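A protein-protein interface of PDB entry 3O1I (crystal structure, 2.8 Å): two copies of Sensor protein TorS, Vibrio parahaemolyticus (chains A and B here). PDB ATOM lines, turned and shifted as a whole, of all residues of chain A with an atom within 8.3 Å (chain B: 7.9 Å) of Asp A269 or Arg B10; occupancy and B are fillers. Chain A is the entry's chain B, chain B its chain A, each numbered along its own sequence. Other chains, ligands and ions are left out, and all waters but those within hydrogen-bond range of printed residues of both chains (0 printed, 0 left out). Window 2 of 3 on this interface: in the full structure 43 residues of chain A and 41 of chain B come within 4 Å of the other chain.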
ATOM      1  N   ALA A   5       4.866  17.209  31.338  1.00  0.00           N
ATOM      2  CA  ALA A   5       4.323  17.523  30.028  1.00  0.00           C
ATOM      3  C   ALA A   5       2.956  16.871  29.870  1.00  0.00           C
ATOM      4  O   ALA A   5       2.103  17.370  29.139  1.00  0.00           O
ATOM      5  CB  ALA A   5       5.269  17.023  28.947  1.00  0.00           C
ATOM      6  N   MET A   6       2.753  15.754  30.563  1.00  0.00           N
ATOM      7  CA  MET A   6       1.494  15.024  30.502  1.00  0.00           C
ATOM      8  C   MET A   6       0.308  15.858  30.971  1.00  0.00           C
ATOM      9  O   MET A   6      -0.533  16.251  30.163  1.00  0.00           O
ATOM     10  CB  MET A   6       1.574  13.744  31.342  1.00  0.00           C
ATOM     11  CG  MET A   6       2.529  12.674  30.807  1.00  0.00           C
ATOM     12  SD  MET A   6       4.308  13.029  30.980  1.00  0.00           S
ATOM     13  CE  MET A   6       4.721  12.113  32.495  1.00  0.00           C
ATOM     14  N   ALA A   9      -0.389  18.445  28.433  1.00  0.00           N
ATOM     15  CA  ALA A   9      -0.896  17.972  27.156  1.00  0.00           C
ATOM     16  C   ALA A   9      -2.323  17.461  27.257  1.00  0.00           C
ATOM     17  O   ALA A   9      -3.074  17.533  26.288  1.00  0.00           O
ATOM     18  CB  ALA A   9       0.008  16.879  26.615  1.00  0.00           C
ATOM     19  N   ARG A  10      -2.695  16.936  28.422  1.00  0.00           N
ATOM     20  CA  ARG A  10      -4.043  16.410  28.626  1.00  0.00           C
ATOM     21  C   ARG A  10      -5.002  17.560  28.886  1.00  0.00           C
ATOM     22  O   ARG A  10      -6.127  17.575  28.386  1.00  0.00           O
ATOM     23  CB  ARG A  10      -4.079  15.452  29.822  1.00  0.00           C
ATOM     24  CG  ARG A  10      -3.930  16.138  31.182  1.00  0.00           C
ATOM     25  CD  ARG A  10      -5.098  15.799  32.103  1.00  0.00           C
ATOM     26  NE  ARG A  10      -5.149  14.373  32.406  1.00  0.00           N
ATOM     27  CZ  ARG A  10      -4.252  13.740  33.152  1.00  0.00           C
ATOM     28  NH1 ARG A  10      -3.241  14.416  33.675  1.00  0.00           N
ATOM     29  NH2 ARG A  10      -4.355  12.436  33.361  1.00  0.00           N
ATOM     30  N   SER A  13      -5.597  18.967  25.421  1.00  0.00           N
ATOM     31  CA  SER A  13      -6.439  18.073  24.624  1.00  0.00           C
ATOM     32  C   SER A  13      -7.887  18.084  25.103  1.00  0.00           C
ATOM     33  O   SER A  13      -8.801  17.763  24.339  1.00  0.00           O
ATOM     34  CB  SER A  13      -5.900  16.643  24.672  1.00  0.00           C
ATOM     35  OG  SER A  13      -4.608  16.567  24.090  1.00  0.00           O
ATOM     36  N   LEU A  56       3.638  23.939  28.475  1.00  0.00           N
ATOM     37  CA  LEU A  56       3.944  22.765  27.668  1.00  0.00           C
ATOM     38  C   LEU A  56       4.970  23.087  26.590  1.00  0.00           C
ATOM     39  O   LEU A  56       5.815  22.260  26.257  1.00  0.00           O
ATOM     40  CB  LEU A  56       2.668  22.241  27.009  1.00  0.00           C
ATOM     41  CG  LEU A  56       2.835  21.022  26.102  1.00  0.00           C
ATOM     42  CD1 LEU A  56       3.207  19.808  26.934  1.00  0.00           C
ATOM     43  CD2 LEU A  56       1.539  20.775  25.352  1.00  0.00           C
ATOM     44  N   SER A  60       9.959  21.877  25.808  1.00  0.00           N
ATOM     45  CA  SER A  60      10.547  21.200  24.657  1.00  0.00           C
ATOM     46  C   SER A  60      11.366  22.168  23.817  1.00  0.00           C
ATOM     47  O   SER A  60      10.815  23.064  23.181  1.00  0.00           O
ATOM     48  CB  SER A  60       9.457  20.570  23.789  1.00  0.00           C
ATOM     49  OG  SER A  60      10.022  19.993  22.625  1.00  0.00           O
ATOM     50  N   LEU A  65       9.273  21.969  15.912  1.00  0.00           N
ATOM     51  CA  LEU A  65       7.988  21.712  16.549  1.00  0.00           C
ATOM     52  C   LEU A  65       7.388  22.962  17.171  1.00  0.00           C
ATOM     53  O   LEU A  65       6.171  23.138  17.155  1.00  0.00           O
ATOM     54  CB  LEU A  65       8.097  20.619  17.622  1.00  0.00           C
ATOM     55  CG  LEU A  65       8.012  19.158  17.162  1.00  0.00           C
ATOM     56  CD1 LEU A  65       7.531  18.306  18.327  1.00  0.00           C
ATOM     57  CD2 LEU A  65       7.045  19.012  15.994  1.00  0.00           C
ATOM     58  N   ASN A 261      -3.465  19.390  18.956  1.00  0.00           N
ATOM     59  CA  ASN A 261      -3.222  18.257  19.826  1.00  0.00           C
ATOM     60  C   ASN A 261      -2.178  17.338  19.216  1.00  0.00           C
ATOM     61  O   ASN A 261      -1.356  16.779  19.928  1.00  0.00           O
ATOM     62  CB  ASN A 261      -4.506  17.475  20.067  1.00  0.00           C
ATOM     63  CG  ASN A 261      -5.533  18.271  20.821  1.00  0.00           C
ATOM     64  OD1 ASN A 261      -5.227  18.879  21.847  1.00  0.00           O
ATOM     65  ND2 ASN A 261      -6.769  18.266  20.329  1.00  0.00           N
ATOM     66  N   SER A 262      -2.206  17.178  17.900  1.00  0.00           N
ATOM     67  CA  SER A 262      -1.231  16.315  17.244  1.00  0.00           C
ATOM     68  C   SER A 262       0.199  16.810  17.482  1.00  0.00           C
ATOM     69  O   SER A 262       1.133  16.020  17.584  1.00  0.00           O
ATOM     70  CB  SER A 262      -1.499  16.243  15.734  1.00  0.00           C
ATOM     71  OG  SER A 262      -0.542  15.415  15.082  1.00  0.00           O
ATOM     72  N   THR A 263       0.363  18.124  17.568  1.00  0.00           N
ATOM     73  CA  THR A 263       1.676  18.703  17.787  1.00  0.00           C
ATOM     74  C   THR A 263       2.064  18.616  19.253  1.00  0.00           C
ATOM     75  O   THR A 263       3.150  18.144  19.571  1.00  0.00           O
ATOM     76  CB  THR A 263       1.726  20.173  17.306  1.00  0.00           C
ATOM     77  OG1 THR A 263       1.608  20.201  15.879  1.00  0.00           O
ATOM     78  CG2 THR A 263       3.040  20.841  17.711  1.00  0.00           C
ATOM     79  N   VAL A 264       1.184  19.054  20.146  1.00  0.00           N
ATOM     80  CA  VAL A 264       1.500  18.988  21.569  1.00  0.00           C
ATOM     81  C   VAL A 264       1.900  17.567  21.967  1.00  0.00           C
ATOM     82  O   VAL A 264       2.781  17.378  22.806  1.00  0.00           O
ATOM     83  CB  VAL A 264       0.315  19.432  22.448  1.00  0.00           C
ATOM     84  CG1 VAL A 264      -0.325  20.668  21.857  1.00  0.00           C
ATOM     85  CG2 VAL A 264      -0.682  18.307  22.601  1.00  0.00           C
ATOM     86  N   ASN A 265       1.252  16.573  21.363  1.00  0.00           N
ATOM     87  CA  ASN A 265       1.567  15.177  21.653  1.00  0.00           C
ATOM     88  C   ASN A 265       2.969  14.843  21.165  1.00  0.00           C
ATOM     89  O   ASN A 265       3.684  14.068  21.803  1.00  0.00           O
ATOM     90  CB  ASN A 265       0.559  14.237  20.989  1.00  0.00           C
ATOM     91  CG  ASN A 265      -0.692  14.053  21.817  1.00  0.00           C
ATOM     92  OD1 ASN A 265      -0.840  14.644  22.893  1.00  0.00           O
ATOM     93  ND2 ASN A 265      -1.606  13.231  21.324  1.00  0.00           N
ATOM     94  N   LYS A 266       3.357  15.416  20.030  1.00  0.00           N
ATOM     95  CA  LYS A 266       4.687  15.171  19.504  1.00  0.00           C
ATOM     96  C   LYS A 266       5.720  15.872  20.380  1.00  0.00           C
ATOM     97  O   LYS A 266       6.878  15.473  20.422  1.00  0.00           O
ATOM     98  CB  LYS A 266       4.793  15.657  18.056  1.00  0.00           C
ATOM     99  CG  LYS A 266       4.080  14.746  17.076  1.00  0.00           C
ATOM    100  CD  LYS A 266       4.501  14.997  15.636  1.00  0.00           C
ATOM    101  CE  LYS A 266       4.003  16.336  15.126  1.00  0.00           C
ATOM    102  NZ  LYS A 266       4.286  16.492  13.674  1.00  0.00           N
ATOM    103  N   LEU A 267       5.291  16.918  21.082  1.00  0.00           N
ATOM    104  CA  LEU A 267       6.186  17.646  21.971  1.00  0.00           C
ATOM    105  C   LEU A 267       6.371  16.812  23.224  1.00  0.00           C
ATOM    106  O   LEU A 267       7.462  16.744  23.777  1.00  0.00           O
ATOM    107  CB  LEU A 267       5.607  19.012  22.347  1.00  0.00           C
ATOM    108  CG  LEU A 267       5.585  20.104  21.275  1.00  0.00           C
ATOM    109  CD1 LEU A 267       5.139  21.403  21.935  1.00  0.00           C
ATOM    110  CD2 LEU A 267       6.957  20.282  20.640  1.00  0.00           C
ATOM    111  N   VAL A 268       5.292  16.184  23.668  1.00  0.00           N
ATOM    112  CA  VAL A 268       5.336  15.336  24.847  1.00  0.00           C
ATOM    113  C   VAL A 268       6.303  14.181  24.606  1.00  0.00           C
ATOM    114  O   VAL A 268       7.167  13.899  25.436  1.00  0.00           O
ATOM    115  CB  VAL A 268       3.938  14.778  25.168  1.00  0.00           C
ATOM    116  CG1 VAL A 268       4.013  13.768  26.304  1.00  0.00           C
ATOM    117  CG2 VAL A 268       3.020  15.921  25.538  1.00  0.00           C
ATOM    118  N   ASP A 269       6.158  13.517  23.465  1.00  0.00           N
ATOM    119  CA  ASP A 269       7.036  12.406  23.133  1.00  0.00           C
ATOM    120  C   ASP A 269       8.498  12.839  23.105  1.00  0.00           C
ATOM    121  O   ASP A 269       9.382  12.073  23.485  1.00  0.00           O
ATOM    122  CB  ASP A 269       6.670  11.819  21.771  1.00  0.00           C
ATOM    123  CG  ASP A 269       5.309  11.167  21.762  1.00  0.00           C
ATOM    124  OD1 ASP A 269       4.680  11.082  22.841  1.00  0.00           O
ATOM    125  OD2 ASP A 269       4.874  10.739  20.671  1.00  0.00           O
ATOM    126  N   ASP A 270       8.747  14.063  22.651  1.00  0.00           N
ATOM    127  CA  ASP A 270      10.107  14.588  22.569  1.00  0.00           C
ATOM    128  C   ASP A 270      10.691  14.786  23.973  1.00  0.00           C
ATOM    129  O   ASP A 270      11.761  14.268  24.287  1.00  0.00           O
ATOM    130  CB  ASP A 270      10.104  15.925  21.813  1.00  0.00           C
ATOM    131  CG  ASP A 270      11.395  16.177  21.044  1.00  0.00           C
ATOM    132  OD1 ASP A 270      11.623  17.337  20.628  1.00  0.00           O
ATOM    133  OD2 ASP A 270      12.173  15.218  20.841  1.00  0.00           O
ATOM    134  N   SER A 271       9.980  15.530  24.816  1.00  0.00           N
ATOM    135  CA  SER A 271      10.445  15.796  26.171  1.00  0.00           C
ATOM    136  C   SER A 271      10.608  14.516  26.985  1.00  0.00           C
ATOM    137  O   SER A 271      11.696  14.225  27.481  1.00  0.00           O
ATOM    138  CB  SER A 271       9.478  16.736  26.895  1.00  0.00           C
ATOM    139  OG  SER A 271       8.268  16.075  27.222  1.00  0.00           O
ATOM    140  N   ASN A 272       9.527  13.757  27.128  1.00  0.00           N
ATOM    141  CA  ASN A 272       9.575  12.515  27.891  1.00  0.00           C
ATOM    142  C   ASN A 272       9.798  11.325  26.964  1.00  0.00           C
ATOM    143  O   ASN A 272      10.975  10.962  26.743  1.00  0.00           O
ATOM    144  CB  ASN A 272       8.269  12.316  28.672  1.00  0.00           C
ATOM    145  CG  ASN A 272       8.002  13.434  29.668  1.00  0.00           C
ATOM    146  OD1 ASN A 272       8.763  13.640  30.615  1.00  0.00           O
ATOM    147  ND2 ASN A 272       6.912  14.164  29.456  1.00  0.00           N
ATOM    148  N   SER B   4       1.580   1.602  30.663  1.00  0.00           N
ATOM    149  CA  SER B   4       1.340   1.392  29.230  1.00  0.00           C
ATOM    150  C   SER B   4      -0.034   1.940  28.863  1.00  0.00           C
ATOM    151  O   SER B   4      -0.443   1.921  27.696  1.00  0.00           O
ATOM    152  CB  SER B   4       1.392  -0.103  28.900  1.00  0.00           C
ATOM    153  OG  SER B   4       0.408  -0.829  29.623  1.00  0.00           O
ATOM    154  N   ALA B   5      -0.739   2.412  29.887  1.00  0.00           N
ATOM    155  CA  ALA B   5      -2.065   2.983  29.740  1.00  0.00           C
ATOM    156  C   ALA B   5      -2.013   4.214  28.851  1.00  0.00           C
ATOM    157  O   ALA B   5      -2.877   4.414  28.000  1.00  0.00           O
ATOM    158  CB  ALA B   5      -2.621   3.348  31.106  1.00  0.00           C
ATOM    159  N   MET B   6      -0.986   5.033  29.047  1.00  0.00           N
ATOM    160  CA  MET B   6      -0.813   6.260  28.274  1.00  0.00           C
ATOM    161  C   MET B   6      -0.656   5.981  26.782  1.00  0.00           C
ATOM    162  O   MET B   6      -0.811   6.874  25.953  1.00  0.00           O
ATOM    163  CB  MET B   6       0.400   7.041  28.797  1.00  0.00           C
ATOM    164  CG  MET B   6       0.392   7.230  30.317  1.00  0.00           C
ATOM    165  SD  MET B   6       1.748   8.231  30.956  1.00  0.00           S
ATOM    166  CE  MET B   6       0.903   9.858  31.099  1.00  0.00           C
ATOM    167  N   ILE B   7      -0.350   4.734  26.448  1.00  0.00           N
ATOM    168  CA  ILE B   7      -0.184   4.329  25.055  1.00  0.00           C
ATOM    169  C   ILE B   7      -1.571   4.155  24.421  1.00  0.00           C
ATOM    170  O   ILE B   7      -1.803   4.547  23.275  1.00  0.00           O
ATOM    171  CB  ILE B   7       0.583   2.989  24.959  1.00  0.00           C
ATOM    172  CG1 ILE B   7       1.809   3.022  25.879  1.00  0.00           C
ATOM    173  CG2 ILE B   7       1.015   2.739  23.524  1.00  0.00           C
ATOM    174  CD1 ILE B   7       2.522   1.690  26.005  1.00  0.00           C
ATOM    175  N   GLU B   8      -2.488   3.556  25.176  1.00  0.00           N
ATOM    176  CA  GLU B   8      -3.849   3.345  24.698  1.00  0.00           C
ATOM    177  C   GLU B   8      -4.607   4.662  24.775  1.00  0.00           C
ATOM    178  O   GLU B   8      -5.234   5.087  23.806  1.00  0.00           O
ATOM    179  CB  GLU B   8      -4.569   2.289  25.551  1.00  0.00           C
ATOM    180  CG  GLU B   8      -4.111   0.856  25.318  1.00  0.00           C
ATOM    181  CD  GLU B   8      -4.495   0.326  23.946  1.00  0.00           C
ATOM    182  OE1 GLU B   8      -4.177   0.981  22.934  1.00  0.00           O
ATOM    183  OE2 GLU B   8      -5.108  -0.756  23.877  1.00  0.00           O
ATOM    184  N   ALA B   9      -4.533   5.302  25.938  1.00  0.00           N
ATOM    185  CA  ALA B   9      -5.209   6.565  26.180  1.00  0.00           C
ATOM    186  C   ALA B   9      -5.066   7.544  25.028  1.00  0.00           C
ATOM    187  O   ALA B   9      -6.025   8.225  24.671  1.00  0.00           O
ATOM    188  CB  ALA B   9      -4.683   7.200  27.451  1.00  0.00           C
ATOM    189  N   ARG B  10      -3.872   7.624  24.455  1.00  0.00           N
ATOM    190  CA  ARG B  10      -3.635   8.530  23.342  1.00  0.00           C
ATOM    191  C   ARG B  10      -4.501   8.152  22.157  1.00  0.00           C
ATOM    192  O   ARG B  10      -5.258   8.972  21.639  1.00  0.00           O
ATOM    193  CB  ARG B  10      -2.165   8.498  22.928  1.00  0.00           C
ATOM    194  CG  ARG B  10      -1.893   9.152  21.574  1.00  0.00           C
ATOM    195  CD  ARG B  10      -0.521   9.781  21.545  1.00  0.00           C
ATOM    196  NE  ARG B  10      -0.373  10.717  22.657  1.00  0.00           N
ATOM    197  CZ  ARG B  10       0.776  11.291  23.011  1.00  0.00           C
ATOM    198  NH1 ARG B  10       1.893  11.030  22.340  1.00  0.00           N
ATOM    199  NH2 ARG B  10       0.808  12.115  24.052  1.00  0.00           N
ATOM    200  N   GLN B  11      -4.375   6.903  21.724  1.00  0.00           N
ATOM    201  CA  GLN B  11      -5.152   6.413  20.602  1.00  0.00           C
ATOM    202  C   GLN B  11      -6.616   6.774  20.794  1.00  0.00           C
ATOM    203  O   GLN B  11      -7.251   7.301  19.880  1.00  0.00           O
ATOM    204  CB  GLN B  11      -4.976   4.906  20.478  1.00  0.00           C
ATOM    205  CG  GLN B  11      -3.598   4.520  19.978  1.00  0.00           C
ATOM    206  CD  GLN B  11      -3.298   3.062  20.202  1.00  0.00           C
ATOM    207  OE1 GLN B  11      -3.157   2.618  21.342  1.00  0.00           O
ATOM    208  NE2 GLN B  11      -3.203   2.301  19.116  1.00  0.00           N
ATOM    209  N   VAL B  12      -7.138   6.507  21.990  1.00  0.00           N
ATOM    210  CA  VAL B  12      -8.520   6.834  22.312  1.00  0.00           C
ATOM    211  C   VAL B  12      -8.762   8.300  21.997  1.00  0.00           C
ATOM    212  O   VAL B  12      -9.761   8.655  21.379  1.00  0.00           O
ATOM    213  CB  VAL B  12      -8.838   6.585  23.806  1.00  0.00           C
ATOM    214  CG1 VAL B  12     -10.191   7.180  24.162  1.00  0.00           C
ATOM    215  CG2 VAL B  12      -8.855   5.091  24.083  1.00  0.00           C
ATOM    216  N   SER B  13      -7.835   9.148  22.412  1.00  0.00           N
ATOM    217  CA  SER B  13      -7.949  10.574  22.164  1.00  0.00           C
ATOM    218  C   SER B  13      -7.838  10.889  20.669  1.00  0.00           C
ATOM    219  O   SER B  13      -8.416  11.867  20.176  1.00  0.00           O
ATOM    220  CB  SER B  13      -6.859  11.317  22.933  1.00  0.00           C
ATOM    221  OG  SER B  13      -7.073  12.712  22.875  1.00  0.00           O
ATOM    222  N   GLU B  14      -7.096  10.054  19.950  1.00  0.00           N
ATOM    223  CA  GLU B  14      -6.908  10.240  18.519  1.00  0.00           C
ATOM    224  C   GLU B  14      -8.185   9.851  17.800  1.00  0.00           C
ATOM    225  O   GLU B  14      -8.615  10.538  16.871  1.00  0.00           O
ATOM    226  CB  GLU B  14      -5.745   9.381  18.022  1.00  0.00           C
ATOM    227  CG  GLU B  14      -4.450   9.648  18.784  1.00  0.00           C
ATOM    228  CD  GLU B  14      -3.300   8.762  18.345  1.00  0.00           C
ATOM    229  OE1 GLU B  14      -3.460   7.517  18.330  1.00  0.00           O
ATOM    230  OE2 GLU B  14      -2.227   9.318  18.027  1.00  0.00           O
ATOM    231  N   LEU B  15      -8.792   8.748  18.237  1.00  0.00           N
ATOM    232  CA  LEU B  15     -10.036   8.272  17.644  1.00  0.00           C
ATOM    233  C   LEU B  15     -11.147   9.241  17.999  1.00  0.00           C
ATOM    234  O   LEU B  15     -11.884   9.694  17.131  1.00  0.00           O
ATOM    235  CB  LEU B  15     -10.379   6.873  18.151  1.00  0.00           C
ATOM    236  CG  LEU B  15      -9.458   5.760  17.644  1.00  0.00           C
ATOM    237  CD1 LEU B  15      -9.882   4.446  18.260  1.00  0.00           C
ATOM    238  CD2 LEU B  15      -9.500   5.678  16.120  1.00  0.00           C
ATOM    239  N   SER B  16     -11.261   9.568  19.279  1.00  0.00           N
ATOM    240  CA  SER B  16     -12.280  10.505  19.707  1.00  0.00           C
ATOM    241  C   SER B  16     -12.366  11.658  18.720  1.00  0.00           C
ATOM    242  O   SER B  16     -13.459  12.066  18.322  1.00  0.00           O
ATOM    243  CB  SER B  16     -11.956  11.049  21.092  1.00  0.00           C
ATOM    244  OG  SER B  16     -12.052  10.029  22.062  1.00  0.00           O
ATOM    245  N   THR B  17     -11.214  12.177  18.305  1.00  0.00           N
ATOM    246  CA  THR B  17     -11.211  13.301  17.374  1.00  0.00           C
ATOM    247  C   THR B  17     -11.584  12.908  15.945  1.00  0.00           C
ATOM    248  O   THR B  17     -11.994  13.754  15.162  1.00  0.00           O
ATOM    249  CB  THR B  17      -9.840  14.050  17.364  1.00  0.00           C
ATOM    250  OG1 THR B  17      -8.772  13.109  17.180  1.00  0.00           O
ATOM    251  CG2 THR B  17      -9.637  14.821  18.673  1.00  0.00           C
ATOM    252  N   HIS B  52      -9.433  -0.284  22.186  1.00  0.00           N
ATOM    253  CA  HIS B  52      -8.521   0.465  23.029  1.00  0.00           C
ATOM    254  C   HIS B  52      -9.150   0.789  24.386  1.00  0.00           C
ATOM    255  O   HIS B  52      -8.470   0.775  25.408  1.00  0.00           O
ATOM    256  CB  HIS B  52      -8.054   1.741  22.318  1.00  0.00           C
ATOM    257  CG  HIS B  52      -7.330   1.479  21.031  1.00  0.00           C
ATOM    258  ND1 HIS B  52      -6.461   0.422  20.869  1.00  0.00           N
ATOM    259  CD2 HIS B  52      -7.332   2.147  19.851  1.00  0.00           C
ATOM    260  CE1 HIS B  52      -5.959   0.447  19.646  1.00  0.00           C
ATOM    261  NE2 HIS B  52      -6.470   1.484  19.007  1.00  0.00           N
ATOM    262  N   LEU B  56      -7.564  -0.448  27.954  1.00  0.00           N
ATOM    263  CA  LEU B  56      -7.321   0.543  28.982  1.00  0.00           C
ATOM    264  C   LEU B  56      -8.088   0.193  30.251  1.00  0.00           C
ATOM    265  O   LEU B  56      -7.844   0.760  31.311  1.00  0.00           O
ATOM    266  CB  LEU B  56      -7.742   1.922  28.471  1.00  0.00           C
ATOM    267  CG  LEU B  56      -7.315   3.135  29.297  1.00  0.00           C
ATOM    268  CD1 LEU B  56      -5.793   3.187  29.391  1.00  0.00           C
ATOM    269  CD2 LEU B  56      -7.853   4.399  28.647  1.00  0.00           C
ATOM    270  N   ASN B 261     -13.108  10.824  27.706  1.00  0.00           N
ATOM    271  CA  ASN B 261     -11.688  11.082  27.886  1.00  0.00           C
ATOM    272  C   ASN B 261     -11.347  11.579  29.281  1.00  0.00           C
ATOM    273  O   ASN B 261     -10.297  11.245  29.819  1.00  0.00           O
ATOM    274  CB  ASN B 261     -11.218  12.055  26.822  1.00  0.00           C
ATOM    275  CG  ASN B 261     -11.229  11.428  25.450  1.00  0.00           C
ATOM    276  OD1 ASN B 261     -10.321  10.683  25.098  1.00  0.00           O
ATOM    277  ND2 ASN B 261     -12.276  11.700  24.676  1.00  0.00           N
ATOM    278  N   VAL B 264     -10.911   8.436  31.047  1.00  0.00           N
ATOM    279  CA  VAL B 264      -9.737   7.640  30.672  1.00  0.00           C
ATOM    280  C   VAL B 264      -8.461   8.237  31.248  1.00  0.00           C
ATOM    281  O   VAL B 264      -7.451   7.551  31.382  1.00  0.00           O
ATOM    282  CB  VAL B 264      -9.569   7.525  29.132  1.00  0.00           C
ATOM    283  CG1 VAL B 264     -10.928   7.296  28.476  1.00  0.00           C
ATOM    284  CG2 VAL B 264      -8.867   8.756  28.578  1.00  0.00           C
ATOM    285  N   ASN B 265      -8.526   9.526  31.575  1.00  0.00           N
ATOM    286  CA  ASN B 265      -7.402  10.250  32.160  1.00  0.00           C
ATOM    287  C   ASN B 265      -7.221   9.832  33.600  1.00  0.00           C
ATOM    288  O   ASN B 265      -6.118   9.498  34.023  1.00  0.00           O
ATOM    289  CB  ASN B 265      -7.641  11.759  32.128  1.00  0.00           C
ATOM    290  CG  ASN B 265      -7.275  12.373  30.803  1.00  0.00           C
ATOM    291  OD1 ASN B 265      -6.598  11.743  29.981  1.00  0.00           O
ATOM    292  ND2 ASN B 265      -7.704  13.616  30.587  1.00  0.00           N
ATOM    293  N   VAL B 268      -5.788   6.556  33.760  1.00  0.00           N
ATOM    294  CA  VAL B 268      -4.399   6.414  33.339  1.00  0.00           C
ATOM    295  C   VAL B 268      -3.478   6.883  34.476  1.00  0.00           C
ATOM    296  O   VAL B 268      -2.259   6.724  34.410  1.00  0.00           O
ATOM    297  CB  VAL B 268      -4.115   7.231  32.042  1.00  0.00           C
ATOM    298  CG1 VAL B 268      -3.838   8.683  32.380  1.00  0.00           C
ATOM    299  CG2 VAL B 268      -2.953   6.621  31.280  1.00  0.00           C
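ND2 of Asn A265 lies close to NE of Arg B10, 3.1 Å away.
The side-chain carboxylate (OD1) of Asp A269 is in salt-bridge range of the guanidinium group (NH1) of Arg B10, 2.8 Å away.
The guanidinium group (NE) of Arg A10 sits close to the side-chain amide nitrogen (ND2) of Asn B265 (3.2 Å).
The side-chain sulfur (SD) of Met A6 is in hydrogen-bond range of the side-chain amide nitrogen (ND2) of Asn A272 (3.2 Å).
Among the printed residues, pairs that only touch across the chains: Met A6 with Met B6 and Arg A10 with Val B268.
No residue of chain A comes within 4 Å of Ala B9.
Of the printed residues of chain A, Asn B265 touches Arg A10 (3.2 Å).
Of the printed residues of chain B, Asn A265 touches Arg B10.
Of the printed residues of chain B, Arg A10 touches Asn B265 (3.2 Å) and Val B268 (3.9 Å).
Printed residues of chain A within 4 Å of Met B6: Met A6 (3.3 Å).
Val A268 touches none of the printed residues of chain B.
The nearest residue of chain A that does not touch Arg B10 is Val A268 (4.3 Å).
The nearest printed residue of chain A that does not touch Val B268 is Met A6 (7.5 Å).
Of the 20 printed residues of chain B, 4 touch a printed residue of chain A.
Among the printed residues, 5 pairs touch across the chains.
Among the printed residues, Asp or Glu carboxylates within 4 Å of a Lys or Arg side-chain nitrogen of the other chain: Asp A269 with Arg B10 (2.8 Å).
Met A6 touches its own counterpart, Met B6.
Arg A10 touches Asn B265, and with the chains exchanged Asn A265 touches Arg B10.
Arg A10 touches Val B268, but with the chains exchanged Val A268 does not touch Arg B10 (4.3 Å).
Of the 5 pairs that touch across the chains among the printed residues, 3 have their exchanged pair printed and touching as well.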
